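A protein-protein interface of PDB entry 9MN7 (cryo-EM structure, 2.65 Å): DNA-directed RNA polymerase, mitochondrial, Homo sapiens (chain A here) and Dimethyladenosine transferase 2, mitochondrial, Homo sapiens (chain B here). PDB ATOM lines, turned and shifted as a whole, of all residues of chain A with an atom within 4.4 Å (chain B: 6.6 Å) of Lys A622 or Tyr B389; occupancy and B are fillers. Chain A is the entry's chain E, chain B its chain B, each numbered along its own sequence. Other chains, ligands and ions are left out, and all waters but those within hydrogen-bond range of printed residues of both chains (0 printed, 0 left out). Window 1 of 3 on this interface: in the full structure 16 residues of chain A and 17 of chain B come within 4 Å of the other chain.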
ATOM      1  N   ALA A 492      31.025   7.193  10.626  1.00  0.00           N
ATOM      2  CA  ALA A 492      29.987   6.166  10.559  1.00  0.00           C
ATOM      3  C   ALA A 492      28.603   6.776  10.735  1.00  0.00           C
ATOM      4  O   ALA A 492      27.704   6.553   9.918  1.00  0.00           O
ATOM      5  CB  ALA A 492      30.245   5.092  11.615  1.00  0.00           C
ATOM      6  N   GLY A 494      26.777   9.705   9.844  1.00  0.00           N
ATOM      7  CA  GLY A 494      27.096  10.642   8.793  1.00  0.00           C
ATOM      8  C   GLY A 494      26.867  12.085   9.195  1.00  0.00           C
ATOM      9  O   GLY A 494      26.112  12.404  10.113  1.00  0.00           O
ATOM     10  N   VAL A 605      26.992   4.140  -1.868  1.00  0.00           N
ATOM     11  CA  VAL A 605      27.868   4.210  -0.704  1.00  0.00           C
ATOM     12  C   VAL A 605      27.294   5.141   0.356  1.00  0.00           C
ATOM     13  O   VAL A 605      27.418   4.863   1.556  1.00  0.00           O
ATOM     14  CB  VAL A 605      29.279   4.644  -1.143  1.00  0.00           C
ATOM     15  CG1 VAL A 605      30.230   4.747   0.041  1.00  0.00           C
ATOM     16  CG2 VAL A 605      29.827   3.680  -2.176  1.00  0.00           C
ATOM     17  N   LEU A 606      26.612   6.208  -0.055  1.00  0.00           N
ATOM     18  CA  LEU A 606      26.041   7.166   0.875  1.00  0.00           C
ATOM     19  C   LEU A 606      24.529   7.166   0.713  1.00  0.00           C
ATOM     20  O   LEU A 606      24.004   6.923  -0.376  1.00  0.00           O
ATOM     21  CB  LEU A 606      26.597   8.575   0.633  1.00  0.00           C
ATOM     22  CG  LEU A 606      28.108   8.726   0.827  1.00  0.00           C
ATOM     23  CD1 LEU A 606      28.550  10.168   0.597  1.00  0.00           C
ATOM     24  CD2 LEU A 606      28.543   8.218   2.185  1.00  0.00           C
ATOM     25  N   TYR A 607      23.827   7.443   1.811  1.00  0.00           N
ATOM     26  CA  TYR A 607      22.371   7.482   1.806  1.00  0.00           C
ATOM     27  C   TYR A 607      21.877   8.761   2.456  1.00  0.00           C
ATOM     28  O   TYR A 607      22.499   9.280   3.386  1.00  0.00           O
ATOM     29  CB  TYR A 607      21.731   6.291   2.538  1.00  0.00           C
ATOM     30  CG  TYR A 607      22.125   4.904   2.071  1.00  0.00           C
ATOM     31  CD1 TYR A 607      23.373   4.360   2.357  1.00  0.00           C
ATOM     32  CD2 TYR A 607      21.232   4.135   1.343  1.00  0.00           C
ATOM     33  CE1 TYR A 607      23.711   3.090   1.925  1.00  0.00           C
ATOM     34  CE2 TYR A 607      21.560   2.875   0.908  1.00  0.00           C
ATOM     35  CZ  TYR A 607      22.797   2.355   1.200  1.00  0.00           C
ATOM     36  OH  TYR A 607      23.111   1.094   0.759  1.00  0.00           O
ATOM     37  N   VAL A 609      19.483   9.922   4.863  1.00  0.00           N
ATOM     38  CA  VAL A 609      18.561   9.692   5.966  1.00  0.00           C
ATOM     39  C   VAL A 609      18.125  11.045   6.505  1.00  0.00           C
ATOM     40  O   VAL A 609      18.761  12.071   6.239  1.00  0.00           O
ATOM     41  CB  VAL A 609      19.195   8.821   7.065  1.00  0.00           C
ATOM     42  CG1 VAL A 609      19.551   7.450   6.512  1.00  0.00           C
ATOM     43  CG2 VAL A 609      20.424   9.498   7.638  1.00  0.00           C
ATOM     44  N   ILE A 620      20.858  14.066   6.503  1.00  0.00           N
ATOM     45  CA  ILE A 620      22.141  13.500   6.901  1.00  0.00           C
ATOM     46  C   ILE A 620      22.568  12.488   5.848  1.00  0.00           C
ATOM     47  O   ILE A 620      21.774  11.639   5.427  1.00  0.00           O
ATOM     48  CB  ILE A 620      22.052  12.856   8.305  1.00  0.00           C
ATOM     49  CG1 ILE A 620      22.070  13.935   9.393  1.00  0.00           C
ATOM     50  CG2 ILE A 620      23.179  11.863   8.545  1.00  0.00           C
ATOM     51  CD1 ILE A 620      21.969  13.392  10.799  1.00  0.00           C
ATOM     52  N   LEU A 621      23.819  12.587   5.408  1.00  0.00           N
ATOM     53  CA  LEU A 621      24.396  11.635   4.468  1.00  0.00           C
ATOM     54  C   LEU A 621      25.159  10.584   5.263  1.00  0.00           C
ATOM     55  O   LEU A 621      26.294  10.819   5.685  1.00  0.00           O
ATOM     56  CB  LEU A 621      25.309  12.339   3.466  1.00  0.00           C
ATOM     57  CG  LEU A 621      24.636  13.216   2.407  1.00  0.00           C
ATOM     58  CD1 LEU A 621      25.599  13.489   1.266  1.00  0.00           C
ATOM     59  CD2 LEU A 621      23.352  12.583   1.887  1.00  0.00           C
ATOM     60  N   LYS A 622      24.545   9.420   5.436  1.00  0.00           N
ATOM     61  CA  LYS A 622      25.103   8.343   6.237  1.00  0.00           C
ATOM     62  C   LYS A 622      25.711   7.278   5.342  1.00  0.00           C
ATOM     63  O   LYS A 622      25.097   6.900   4.336  1.00  0.00           O
ATOM     64  CB  LYS A 622      24.022   7.717   7.125  1.00  0.00           C
ATOM     65  CG  LYS A 622      24.542   7.139   8.430  1.00  0.00           C
ATOM     66  CD  LYS A 622      23.446   6.415   9.182  1.00  0.00           C
ATOM     67  CE  LYS A 622      23.962   5.826  10.482  1.00  0.00           C
ATOM     68  NZ  LYS A 622      22.946   4.959  11.139  1.00  0.00           N
ATOM     69  N   PRO A 623      26.902   6.781   5.657  1.00  0.00           N
ATOM     70  CA  PRO A 623      27.530   5.773   4.801  1.00  0.00           C
ATOM     71  C   PRO A 623      26.888   4.404   4.952  1.00  0.00           C
ATOM     72  O   PRO A 623      26.095   4.145   5.859  1.00  0.00           O
ATOM     73  CB  PRO A 623      28.982   5.756   5.288  1.00  0.00           C
ATOM     74  CG  PRO A 623      28.887   6.230   6.684  1.00  0.00           C
ATOM     75  CD  PRO A 623      27.853   7.304   6.647  1.00  0.00           C
ATOM     76  N   HIS A 624      27.243   3.528   4.020  1.00  0.00           N
ATOM     77  CA  HIS A 624      26.793   2.147   4.070  1.00  0.00           C
ATOM     78  C   HIS A 624      27.493   1.448   5.234  1.00  0.00           C
ATOM     79  O   HIS A 624      28.694   1.657   5.445  1.00  0.00           O
ATOM     80  CB  HIS A 624      27.122   1.456   2.742  1.00  0.00           C
ATOM     81  CG  HIS A 624      26.426   0.145   2.523  1.00  0.00           C
ATOM     82  ND1 HIS A 624      26.421  -0.877   3.445  1.00  0.00           N
ATOM     83  CD2 HIS A 624      25.742  -0.321   1.451  1.00  0.00           C
ATOM     84  CE1 HIS A 624      25.744  -1.904   2.966  1.00  0.00           C
ATOM     85  NE2 HIS A 624      25.323  -1.593   1.755  1.00  0.00           N
ATOM     86  N   ASN B 318      12.326   1.564  18.406  1.00  0.00           N
ATOM     87  CA  ASN B 318      12.927   2.787  17.883  1.00  0.00           C
ATOM     88  C   ASN B 318      13.424   2.610  16.453  1.00  0.00           C
ATOM     89  O   ASN B 318      13.569   3.598  15.723  1.00  0.00           O
ATOM     90  CB  ASN B 318      14.063   3.243  18.797  1.00  0.00           C
ATOM     91  CG  ASN B 318      15.035   2.126  19.120  1.00  0.00           C
ATOM     92  OD1 ASN B 318      14.654   1.104  19.692  1.00  0.00           O
ATOM     93  ND2 ASN B 318      16.297   2.314  18.756  1.00  0.00           N
ATOM     94  N   ILE B 319      13.695   1.372  16.038  1.00  0.00           N
ATOM     95  CA  ILE B 319      13.961   1.104  14.629  1.00  0.00           C
ATOM     96  C   ILE B 319      12.681   1.271  13.814  1.00  0.00           C
ATOM     97  O   ILE B 319      12.699   1.793  12.693  1.00  0.00           O
ATOM     98  CB  ILE B 319      14.573  -0.301  14.479  1.00  0.00           C
ATOM     99  CG1 ILE B 319      15.955  -0.342  15.130  1.00  0.00           C
ATOM    100  CG2 ILE B 319      14.689  -0.707  13.023  1.00  0.00           C
ATOM    101  CD1 ILE B 319      16.522  -1.738  15.273  1.00  0.00           C
ATOM    102  N   PHE B 320      11.550   0.852  14.388  1.00  0.00           N
ATOM    103  CA  PHE B 320      10.246   0.952  13.733  1.00  0.00           C
ATOM    104  C   PHE B 320       9.822   2.403  13.533  1.00  0.00           C
ATOM    105  O   PHE B 320       9.411   2.790  12.431  1.00  0.00           O
ATOM    106  CB  PHE B 320       9.218   0.192  14.573  1.00  0.00           C
ATOM    107  CG  PHE B 320       7.830   0.193  14.009  1.00  0.00           C
ATOM    108  CD1 PHE B 320       7.520  -0.566  12.897  1.00  0.00           C
ATOM    109  CD2 PHE B 320       6.820   0.914  14.624  1.00  0.00           C
ATOM    110  CE1 PHE B 320       6.235  -0.583  12.384  1.00  0.00           C
ATOM    111  CE2 PHE B 320       5.533   0.899  14.118  1.00  0.00           C
ATOM    112  CZ  PHE B 320       5.239   0.148  13.000  1.00  0.00           C
ATOM    113  N   PHE B 321       9.954   3.226  14.582  1.00  0.00           N
ATOM    114  CA  PHE B 321       9.477   4.609  14.545  1.00  0.00           C
ATOM    115  C   PHE B 321      10.206   5.416  13.484  1.00  0.00           C
ATOM    116  O   PHE B 321       9.599   6.246  12.795  1.00  0.00           O
ATOM    117  CB  PHE B 321       9.668   5.286  15.904  1.00  0.00           C
ATOM    118  CG  PHE B 321       8.592   4.981  16.909  1.00  0.00           C
ATOM    119  CD1 PHE B 321       8.366   3.691  17.327  1.00  0.00           C
ATOM    120  CD2 PHE B 321       7.813   5.987  17.446  1.00  0.00           C
ATOM    121  CE1 PHE B 321       7.408   3.406  18.248  1.00  0.00           C
ATOM    122  CE2 PHE B 321       6.837   5.696  18.374  1.00  0.00           C
ATOM    123  CZ  PHE B 321       6.638   4.407  18.776  1.00  0.00           C
ATOM    124  N   HIS B 322      11.506   5.160  13.316  1.00  0.00           N
ATOM    125  CA  HIS B 322      12.286   5.903  12.336  1.00  0.00           C
ATOM    126  C   HIS B 322      11.900   5.548  10.908  1.00  0.00           C
ATOM    127  O   HIS B 322      12.293   6.252   9.974  1.00  0.00           O
ATOM    128  CB  HIS B 322      13.776   5.664  12.543  1.00  0.00           C
ATOM    129  CG  HIS B 322      14.630   6.767  12.007  1.00  0.00           C
ATOM    130  ND1 HIS B 322      14.511   8.068  12.442  1.00  0.00           N
ATOM    131  CD2 HIS B 322      15.596   6.772  11.060  1.00  0.00           C
ATOM    132  CE1 HIS B 322      15.377   8.826  11.796  1.00  0.00           C
ATOM    133  NE2 HIS B 322      16.047   8.065  10.949  1.00  0.00           N
ATOM    134  N   LEU B 342      16.171   4.494   3.604  1.00  0.00           N
ATOM    135  CA  LEU B 342      16.218   3.900   4.936  1.00  0.00           C
ATOM    136  C   LEU B 342      16.796   2.492   4.999  1.00  0.00           C
ATOM    137  O   LEU B 342      17.116   2.031   6.099  1.00  0.00           O
ATOM    138  CB  LEU B 342      14.810   3.864   5.552  1.00  0.00           C
ATOM    139  CG  LEU B 342      14.163   5.192   5.929  1.00  0.00           C
ATOM    140  CD1 LEU B 342      12.765   4.943   6.444  1.00  0.00           C
ATOM    141  CD2 LEU B 342      14.999   5.880   6.991  1.00  0.00           C
ATOM    142  N   TRP B 387      19.086  -1.826   8.394  1.00  0.00           N
ATOM    143  CA  TRP B 387      18.530  -0.503   8.631  1.00  0.00           C
ATOM    144  C   TRP B 387      19.638   0.538   8.632  1.00  0.00           C
ATOM    145  O   TRP B 387      20.828   0.213   8.645  1.00  0.00           O
ATOM    146  CB  TRP B 387      17.779  -0.447   9.965  1.00  0.00           C
ATOM    147  CG  TRP B 387      16.552  -1.287   9.990  1.00  0.00           C
ATOM    148  CD1 TRP B 387      16.439  -2.556  10.478  1.00  0.00           C
ATOM    149  CD2 TRP B 387      15.256  -0.924   9.509  1.00  0.00           C
ATOM    150  NE1 TRP B 387      15.152  -3.007  10.327  1.00  0.00           N
ATOM    151  CE2 TRP B 387      14.405  -2.024   9.734  1.00  0.00           C
ATOM    152  CE3 TRP B 387      14.731   0.224   8.908  1.00  0.00           C
ATOM    153  CZ2 TRP B 387      13.060  -2.007   9.382  1.00  0.00           C
ATOM    154  CZ3 TRP B 387      13.393   0.236   8.559  1.00  0.00           C
ATOM    155  CH2 TRP B 387      12.575  -0.871   8.797  1.00  0.00           C
ATOM    156  N   LEU B 388      19.225   1.803   8.616  1.00  0.00           N
ATOM    157  CA  LEU B 388      20.112   2.941   8.817  1.00  0.00           C
ATOM    158  C   LEU B 388      19.585   3.859   9.912  1.00  0.00           C
ATOM    159  O   LEU B 388      19.526   5.079   9.750  1.00  0.00           O
ATOM    160  CB  LEU B 388      20.328   3.733   7.528  1.00  0.00           C
ATOM    161  CG  LEU B 388      21.400   3.244   6.550  1.00  0.00           C
ATOM    162  CD1 LEU B 388      20.944   2.056   5.725  1.00  0.00           C
ATOM    163  CD2 LEU B 388      21.866   4.380   5.657  1.00  0.00           C
ATOM    164  N   TYR B 389      19.184   3.280  11.039  1.00  0.00           N
ATOM    165  CA  TYR B 389      18.823   4.068  12.211  1.00  0.00           C
ATOM    166  C   TYR B 389      20.067   4.653  12.869  1.00  0.00           C
ATOM    167  O   TYR B 389      20.978   3.921  13.258  1.00  0.00           O
ATOM    168  CB  TYR B 389      18.040   3.222  13.218  1.00  0.00           C
ATOM    169  CG  TYR B 389      17.659   3.969  14.479  1.00  0.00           C
ATOM    170  CD1 TYR B 389      16.634   4.904  14.473  1.00  0.00           C
ATOM    171  CD2 TYR B 389      18.316   3.726  15.681  1.00  0.00           C
ATOM    172  CE1 TYR B 389      16.279   5.590  15.622  1.00  0.00           C
ATOM    173  CE2 TYR B 389      17.968   4.407  16.837  1.00  0.00           C
ATOM    174  CZ  TYR B 389      16.949   5.336  16.801  1.00  0.00           C
ATOM    175  OH  TYR B 389      16.602   6.011  17.948  1.00  0.00           O
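O of Tyr B389 sits at hydrogen-bond distance from NZ of Lys A622 (3.1 Å).
The backbone carbonyl oxygen (O) of Leu B342 sits at hydrogen-bond distance from the backbone NH (N) of Leu B388 (3.3 Å).
O of Lys A622 sits at hydrogen-bond distance from N of Tyr A607 (2.9 Å).
O of Val A609 sits at hydrogen-bond distance from N of Ile A620, at 2.9 Å.
Leu B388 touches Tyr A607 (CD2 to CD1, 3.6 Å).
Val A609 touches Leu B388.
Lys A622 touches Leu B388.
Of the printed residues of chain B, Tyr A607 touches Leu B388 (3.6 Å).
Printed residues of chain B within 4 Å of Val A609: Leu B388 (3.9 Å).
Ile A620 touches none of the printed residues of chain B.
Of chain B, only Leu B388 (3.7 Å) and Tyr B389 (3.1 Å) come within 4 Å of Lys A622.
Printed residues of chain A within 4 Å of Leu B388: Tyr A607, Val A609 and Lys A622.
Tyr B389 touches just one residue of chain A: Lys A622.
The nearest residue of chain B that does not touch Lys A622 is Trp B387 (5.8 Å).
The nearest printed residue of chain B that does not touch Tyr A607 is Leu B342 (5.6 Å).
Of the 11 printed residues of chain A, 3 touch a printed residue of chain B.
Hydrophobic or aromatic side chains of chain A that line the printed part of chain B: Tyr A607 and Val A609.
Hydrophobic or aromatic side chains of chain B that line the printed part of chain A: Leu B388.
Among the printed residues, 4 pairs touch across the chains.
Among the printed residues, no Asp or Glu carboxylate lies within 4 Å of a Lys or Arg side-chain nitrogen of the other chain.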
